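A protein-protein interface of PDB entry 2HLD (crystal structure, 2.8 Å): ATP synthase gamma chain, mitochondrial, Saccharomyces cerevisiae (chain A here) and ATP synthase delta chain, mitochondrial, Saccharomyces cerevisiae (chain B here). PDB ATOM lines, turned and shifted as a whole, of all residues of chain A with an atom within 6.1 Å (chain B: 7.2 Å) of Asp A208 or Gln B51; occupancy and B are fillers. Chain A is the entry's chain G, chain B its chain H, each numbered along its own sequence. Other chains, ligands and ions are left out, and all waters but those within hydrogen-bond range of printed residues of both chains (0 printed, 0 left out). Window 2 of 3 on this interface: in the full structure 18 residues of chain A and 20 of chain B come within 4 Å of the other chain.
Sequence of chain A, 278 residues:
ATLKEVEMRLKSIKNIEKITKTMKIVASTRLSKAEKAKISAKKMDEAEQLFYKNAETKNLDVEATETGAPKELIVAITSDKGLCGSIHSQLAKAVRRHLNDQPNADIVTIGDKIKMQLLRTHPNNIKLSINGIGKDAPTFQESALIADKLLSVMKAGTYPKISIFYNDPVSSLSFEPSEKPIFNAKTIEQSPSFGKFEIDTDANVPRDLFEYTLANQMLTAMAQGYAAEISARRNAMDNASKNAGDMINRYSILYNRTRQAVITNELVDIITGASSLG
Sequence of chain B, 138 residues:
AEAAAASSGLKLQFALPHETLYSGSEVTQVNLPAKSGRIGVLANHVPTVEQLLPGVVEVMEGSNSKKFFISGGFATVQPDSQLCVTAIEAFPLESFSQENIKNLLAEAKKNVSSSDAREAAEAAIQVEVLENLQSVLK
The side-chain amide nitrogen (NE2) of Gln B51 lies within hydrogen-bond range of the side-chain carboxylate (OD2) of Asp A208, at 3.2 Å.
OD1 of Asp A208 lies within salt-bridge range of NH1 of Arg A207. The side-chain hydroxyl (OG1) of Thr A213 lies within hydrogen-bond range of the backbone carbonyl oxygen (O) of Leu A209, at 2.6 Å. The backbone NH of Leu B52 lies within hydrogen-bond range of the backbone carbonyl oxygen of Gly B73 (2.8 Å).
Val A205 touches Gln B51 (CG2 to NE2, 3.3 Å). C of Asp A208 touches CZ of Phe B74, at 3.9 Å. Leu A209 touches Val B49. Leu A209 touches Phe B74. CE1 of Tyr A212 touches CA of Gly B73 (3.8 Å). CD2 of Tyr A212 touches CD1 of Phe B74, 3.9 Å away.
Of chain B, only Gln B51 (3.2 Å) and Phe B74 (3.9 Å) come within 4 Å of Asp A208. Gln B51 touches two residues of chain A. Of the printed residues of chain A, Gly B73 touches Tyr A212. Printed residues of chain B within 4 Å of Tyr A212: Gly B73 (3.8 Å) and Phe B74 (3.9 Å). Of the printed residues of chain B, Val A205 touches Gln B51. Of the printed residues of chain A, Phe B74 touches Asp A208 (3.9 Å), Leu A209 (3.6 Å) and Tyr A212 (3.9 Å). Glu B50 touches none of the printed residues of chain A. Gly B72 touches none of the printed residues of chain A. The nearest residue of chain A that does not touch Gln B51 is Asn A204 (4.3 Å).
Of the 14 printed residues of chain B, 4 touch a printed residue of chain A. Hydrophobic or aromatic side chains of chain B within 4 Å of the printed part of chain A: Val B49 and Phe B74. Hydrophobic or aromatic side chains of chain A within 4 Å of the printed part of chain B: Val A205, Leu A209 and Tyr A212. Among the printed residues, 7 pairs touch across the chains.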
ATOM      1  N   ALA A 203      20.478 -19.722   3.121  1.00  0.00           N
ATOM      2  CA  ALA A 203      20.093 -20.784   4.067  1.00  0.00           C
ATOM      3  C   ALA A 203      19.903 -20.220   5.477  1.00  0.00           C
ATOM      4  O   ALA A 203      20.737 -19.433   5.970  1.00  0.00           O
ATOM      5  CB  ALA A 203      21.111 -21.935   4.064  1.00  0.00           C
ATOM      6  N   ASN A 204      18.805 -20.651   6.104  1.00  0.00           N
ATOM      7  CA  ASN A 204      18.265 -20.056   7.329  1.00  0.00           C
ATOM      8  C   ASN A 204      19.318 -19.431   8.257  1.00  0.00           C
ATOM      9  O   ASN A 204      19.901 -20.109   9.105  1.00  0.00           O
ATOM     10  CB  ASN A 204      17.385 -21.075   8.066  1.00  0.00           C
ATOM     11  N   VAL A 205      19.568 -18.138   8.055  1.00  0.00           N
ATOM     12  CA  VAL A 205      20.526 -17.368   8.857  1.00  0.00           C
ATOM     13  C   VAL A 205      19.901 -16.847  10.166  1.00  0.00           C
ATOM     14  O   VAL A 205      20.509 -17.031  11.225  1.00  0.00           O
ATOM     15  CB  VAL A 205      21.208 -16.232   8.020  1.00  0.00           C
ATOM     16  CG1 VAL A 205      21.858 -15.158   8.903  1.00  0.00           C
ATOM     17  CG2 VAL A 205      22.218 -16.825   7.050  1.00  0.00           C
ATOM     18  N   PRO A 206      18.712 -16.212  10.115  1.00  0.00           N
ATOM     19  CA  PRO A 206      17.986 -15.853  11.340  1.00  0.00           C
ATOM     20  C   PRO A 206      17.633 -17.048  12.238  1.00  0.00           C
ATOM     21  O   PRO A 206      17.409 -16.839  13.430  1.00  0.00           O
ATOM     22  CB  PRO A 206      16.716 -15.172  10.814  1.00  0.00           C
ATOM     23  CG  PRO A 206      17.101 -14.649   9.499  1.00  0.00           C
ATOM     24  CD  PRO A 206      17.971 -15.741   8.925  1.00  0.00           C
ATOM     25  N   ARG A 207      17.587 -18.266  11.687  1.00  0.00           N
ATOM     26  CA  ARG A 207      17.448 -19.482  12.503  1.00  0.00           C
ATOM     27  C   ARG A 207      18.693 -19.663  13.377  1.00  0.00           C
ATOM     28  O   ARG A 207      18.582 -19.906  14.580  1.00  0.00           O
ATOM     29  CB  ARG A 207      17.196 -20.730  11.633  1.00  0.00           C
ATOM     30  CG  ARG A 207      17.390 -22.102  12.333  1.00  0.00           C
ATOM     31  CD  ARG A 207      17.577 -23.295  11.360  1.00  0.00           C
ATOM     32  NE  ARG A 207      17.854 -24.585  12.025  1.00  0.00           N
ATOM     33  CZ  ARG A 207      19.033 -25.249  12.019  1.00  0.00           C
ATOM     34  NH1 ARG A 207      20.103 -24.774  11.373  1.00  0.00           N
ATOM     35  NH2 ARG A 207      19.136 -26.407  12.672  1.00  0.00           N
ATOM     36  N   ASP A 208      19.869 -19.525  12.770  1.00  0.00           N
ATOM     37  CA  ASP A 208      21.127 -19.778  13.456  1.00  0.00           C
ATOM     38  C   ASP A 208      21.502 -18.627  14.357  1.00  0.00           C
ATOM     39  O   ASP A 208      21.983 -18.842  15.464  1.00  0.00           O
ATOM     40  CB  ASP A 208      22.255 -20.034  12.458  1.00  0.00           C
ATOM     41  CG  ASP A 208      21.992 -21.242  11.577  1.00  0.00           C
ATOM     42  OD1 ASP A 208      21.397 -22.248  12.065  1.00  0.00           O
ATOM     43  OD2 ASP A 208      22.357 -21.258  10.375  1.00  0.00           O
ATOM     44  N   LEU A 209      21.280 -17.406  13.881  1.00  0.00           N
ATOM     45  CA  LEU A 209      21.541 -16.217  14.673  1.00  0.00           C
ATOM     46  C   LEU A 209      20.643 -16.175  15.928  1.00  0.00           C
ATOM     47  O   LEU A 209      20.803 -15.303  16.785  1.00  0.00           O
ATOM     48  CB  LEU A 209      21.355 -14.977  13.803  1.00  0.00           C
ATOM     49  CG  LEU A 209      21.755 -13.578  14.291  1.00  0.00           C
ATOM     50  CD1 LEU A 209      23.193 -13.542  14.811  1.00  0.00           C
ATOM     51  CD2 LEU A 209      21.537 -12.508  13.197  1.00  0.00           C
ATOM     52  N   PHE A 210      19.706 -17.127  16.029  1.00  0.00           N
ATOM     53  CA  PHE A 210      18.830 -17.274  17.198  1.00  0.00           C
ATOM     54  C   PHE A 210      19.297 -18.438  18.049  1.00  0.00           C
ATOM     55  O   PHE A 210      19.434 -18.283  19.263  1.00  0.00           O
ATOM     56  CB  PHE A 210      17.331 -17.409  16.804  1.00  0.00           C
ATOM     57  CG  PHE A 210      16.508 -18.315  17.720  1.00  0.00           C
ATOM     58  CD1 PHE A 210      16.125 -17.900  18.999  1.00  0.00           C
ATOM     59  CD2 PHE A 210      16.106 -19.586  17.288  1.00  0.00           C
ATOM     60  CE1 PHE A 210      15.369 -18.754  19.842  1.00  0.00           C
ATOM     61  CE2 PHE A 210      15.341 -20.440  18.123  1.00  0.00           C
ATOM     62  CZ  PHE A 210      14.972 -20.025  19.392  1.00  0.00           C
ATOM     63  N   GLU A 211      19.533 -19.593  17.431  1.00  0.00           N
ATOM     64  CA  GLU A 211      20.018 -20.749  18.181  1.00  0.00           C
ATOM     65  C   GLU A 211      21.373 -20.482  18.848  1.00  0.00           C
ATOM     66  O   GLU A 211      21.640 -20.954  19.941  1.00  0.00           O
ATOM     67  CB  GLU A 211      20.070 -21.997  17.310  1.00  0.00           C
ATOM     68  CG  GLU A 211      18.699 -22.493  16.877  1.00  0.00           C
ATOM     69  CD  GLU A 211      18.743 -23.849  16.191  1.00  0.00           C
ATOM     70  OE1 GLU A 211      19.728 -24.132  15.471  1.00  0.00           O
ATOM     71  OE2 GLU A 211      17.784 -24.641  16.360  1.00  0.00           O
ATOM     72  N   TYR A 212      22.203 -19.684  18.194  1.00  0.00           N
ATOM     73  CA  TYR A 212      23.493 -19.271  18.729  1.00  0.00           C
ATOM     74  C   TYR A 212      23.336 -18.243  19.852  1.00  0.00           C
ATOM     75  O   TYR A 212      24.120 -18.239  20.811  1.00  0.00           O
ATOM     76  CB  TYR A 212      24.326 -18.692  17.586  1.00  0.00           C
ATOM     77  CG  TYR A 212      25.691 -18.176  17.951  1.00  0.00           C
ATOM     78  CD1 TYR A 212      26.799 -19.036  17.985  1.00  0.00           C
ATOM     79  CD2 TYR A 212      25.893 -16.820  18.217  1.00  0.00           C
ATOM     80  CE1 TYR A 212      28.072 -18.556  18.293  1.00  0.00           C
ATOM     81  CE2 TYR A 212      27.156 -16.331  18.540  1.00  0.00           C
ATOM     82  CZ  TYR A 212      28.242 -17.202  18.567  1.00  0.00           C
ATOM     83  OH  TYR A 212      29.495 -16.718  18.864  1.00  0.00           O
ATOM     84  N   THR A 213      22.351 -17.356  19.714  1.00  0.00           N
ATOM     85  CA  THR A 213      22.054 -16.369  20.752  1.00  0.00           C
ATOM     86  C   THR A 213      21.388 -17.024  21.980  1.00  0.00           C
ATOM     87  O   THR A 213      21.638 -16.618  23.128  1.00  0.00           O
ATOM     88  CB  THR A 213      21.205 -15.244  20.184  1.00  0.00           C
ATOM     89  OG1 THR A 213      21.865 -14.718  19.031  1.00  0.00           O
ATOM     90  CG2 THR A 213      21.200 -14.047  21.112  1.00  0.00           C
ATOM     91  N   LEU B  32      38.033 -13.529   7.463  1.00  0.00           N
ATOM     92  CA  LEU B  32      37.131 -14.443   8.178  1.00  0.00           C
ATOM     93  C   LEU B  32      36.717 -15.613   7.272  1.00  0.00           C
ATOM     94  O   LEU B  32      36.605 -15.433   6.060  1.00  0.00           O
ATOM     95  CB  LEU B  32      35.869 -13.684   8.627  1.00  0.00           C
ATOM     96  CG  LEU B  32      35.978 -12.241   9.138  1.00  0.00           C
ATOM     97  CD1 LEU B  32      34.636 -11.558   9.093  1.00  0.00           C
ATOM     98  CD2 LEU B  32      36.541 -12.193  10.538  1.00  0.00           C
ATOM     99  N   PRO B  33      36.482 -16.800   7.832  1.00  0.00           N
ATOM    100  CA  PRO B  33      35.976 -17.924   7.039  1.00  0.00           C
ATOM    101  C   PRO B  33      34.442 -17.960   7.012  1.00  0.00           C
ATOM    102  O   PRO B  33      33.822 -18.680   7.793  1.00  0.00           O
ATOM    103  CB  PRO B  33      36.544 -19.145   7.767  1.00  0.00           C
ATOM    104  CG  PRO B  33      36.717 -18.688   9.203  1.00  0.00           C
ATOM    105  CD  PRO B  33      36.683 -17.176   9.241  1.00  0.00           C
ATOM    106  N   ALA B  34      33.851 -17.191   6.103  1.00  0.00           N
ATOM    107  CA  ALA B  34      32.398 -16.995   6.036  1.00  0.00           C
ATOM    108  C   ALA B  34      31.602 -18.212   5.538  1.00  0.00           C
ATOM    109  O   ALA B  34      32.139 -19.322   5.439  1.00  0.00           O
ATOM    110  CB  ALA B  34      32.074 -15.754   5.199  1.00  0.00           C
ATOM    111  N   LYS B  35      30.319 -17.986   5.236  1.00  0.00           N
ATOM    112  CA  LYS B  35      29.374 -19.048   4.853  1.00  0.00           C
ATOM    113  C   LYS B  35      29.969 -20.119   3.920  1.00  0.00           C
ATOM    114  O   LYS B  35      29.915 -21.314   4.231  1.00  0.00           O
ATOM    115  CB  LYS B  35      28.096 -18.443   4.254  1.00  0.00           C
ATOM    116  N   SER B  36      30.548 -19.692   2.795  1.00  0.00           N
ATOM    117  CA  SER B  36      31.207 -20.623   1.870  1.00  0.00           C
ATOM    118  C   SER B  36      32.730 -20.406   1.774  1.00  0.00           C
ATOM    119  O   SER B  36      33.513 -21.357   1.902  1.00  0.00           O
ATOM    120  CB  SER B  36      30.551 -20.569   0.481  1.00  0.00           C
ATOM    121  N   VAL B  49      26.005  -9.415   7.892  1.00  0.00           N
ATOM    122  CA  VAL B  49      25.962 -10.364   8.999  1.00  0.00           C
ATOM    123  C   VAL B  49      26.276 -11.742   8.436  1.00  0.00           C
ATOM    124  O   VAL B  49      25.542 -12.248   7.601  1.00  0.00           O
ATOM    125  CB  VAL B  49      24.569 -10.389   9.717  1.00  0.00           C
ATOM    126  CG1 VAL B  49      24.491 -11.518  10.752  1.00  0.00           C
ATOM    127  CG2 VAL B  49      24.248  -9.044  10.368  1.00  0.00           C
ATOM    128  N   GLU B  50      27.363 -12.350   8.901  1.00  0.00           N
ATOM    129  CA  GLU B  50      27.786 -13.653   8.385  1.00  0.00           C
ATOM    130  C   GLU B  50      28.134 -14.676   9.477  1.00  0.00           C
ATOM    131  O   GLU B  50      28.808 -14.346  10.454  1.00  0.00           O
ATOM    132  CB  GLU B  50      28.974 -13.471   7.428  1.00  0.00           C
ATOM    133  N   GLN B  51      27.664 -15.912   9.295  1.00  0.00           N
ATOM    134  CA  GLN B  51      28.156 -17.050  10.068  1.00  0.00           C
ATOM    135  C   GLN B  51      29.663 -17.145   9.892  1.00  0.00           C
ATOM    136  O   GLN B  51      30.215 -16.603   8.935  1.00  0.00           O
ATOM    137  CB  GLN B  51      27.540 -18.368   9.585  1.00  0.00           C
ATOM    138  CG  GLN B  51      26.099 -18.614   9.990  1.00  0.00           C
ATOM    139  CD  GLN B  51      25.094 -18.190   8.925  1.00  0.00           C
ATOM    140  OE1 GLN B  51      25.314 -17.215   8.196  1.00  0.00           O
ATOM    141  NE2 GLN B  51      23.986 -18.924   8.835  1.00  0.00           N
ATOM    142  N   LEU B  52      30.325 -17.841  10.812  1.00  0.00           N
ATOM    143  CA  LEU B  52      31.727 -18.182  10.664  1.00  0.00           C
ATOM    144  C   LEU B  52      31.858 -19.695  10.742  1.00  0.00           C
ATOM    145  O   LEU B  52      31.406 -20.304  11.703  1.00  0.00           O
ATOM    146  CB  LEU B  52      32.573 -17.506  11.745  1.00  0.00           C
ATOM    147  CG  LEU B  52      32.691 -15.972  11.804  1.00  0.00           C
ATOM    148  CD1 LEU B  52      33.819 -15.558  12.746  1.00  0.00           C
ATOM    149  CD2 LEU B  52      32.896 -15.321  10.429  1.00  0.00           C
ATOM    150  N   LEU B  53      32.447 -20.294   9.708  1.00  0.00           N
ATOM    151  CA  LEU B  53      32.709 -21.741   9.654  1.00  0.00           C
ATOM    152  C   LEU B  53      33.977 -22.059  10.466  1.00  0.00           C
ATOM    153  O   LEU B  53      34.769 -21.150  10.728  1.00  0.00           O
ATOM    154  CB  LEU B  53      32.864 -22.194   8.191  1.00  0.00           C
ATOM    155  N   GLY B  72      34.036 -21.420  15.147  1.00  0.00           N
ATOM    156  CA  GLY B  72      32.921 -20.922  14.357  1.00  0.00           C
ATOM    157  C   GLY B  72      32.144 -19.896  15.163  1.00  0.00           C
ATOM    158  O   GLY B  72      32.535 -19.542  16.282  1.00  0.00           O
ATOM    159  N   GLY B  73      31.036 -19.421  14.607  1.00  0.00           N
ATOM    160  CA  GLY B  73      30.316 -18.326  15.226  1.00  0.00           C
ATOM    161  C   GLY B  73      29.772 -17.371  14.197  1.00  0.00           C
ATOM    162  O   GLY B  73      29.072 -17.799  13.280  1.00  0.00           O
ATOM    163  N   PHE B  74      30.110 -16.089  14.344  1.00  0.00           N
ATOM    164  CA  PHE B  74      29.400 -15.007  13.654  1.00  0.00           C
ATOM    165  C   PHE B  74      30.209 -13.707  13.509  1.00  0.00           C
ATOM    166  O   PHE B  74      30.804 -13.228  14.481  1.00  0.00           O
ATOM    167  CB  PHE B  74      28.076 -14.688  14.386  1.00  0.00           C
ATOM    168  CG  PHE B  74      26.891 -15.473  13.886  1.00  0.00           C
ATOM    169  CD1 PHE B  74      26.599 -16.733  14.399  1.00  0.00           C
ATOM    170  CD2 PHE B  74      26.059 -14.947  12.909  1.00  0.00           C
ATOM    171  CE1 PHE B  74      25.515 -17.466  13.934  1.00  0.00           C
ATOM    172  CE2 PHE B  74      24.959 -15.676  12.442  1.00  0.00           C
ATOM    173  CZ  PHE B  74      24.693 -16.942  12.958  1.00  0.00           C
ATOM    174  N   ALA B  75      30.211 -13.138  12.297  1.00  0.00           N
ATOM    175  CA  ALA B  75      30.692 -11.772  12.077  1.00  0.00           C
ATOM    176  C   ALA B  75      29.532 -10.804  11.762  1.00  0.00           C
ATOM    177  O   ALA B  75      28.553 -11.191  11.110  1.00  0.00           O
ATOM    178  CB  ALA B  75      31.758 -11.731  10.987  1.00  0.00           C
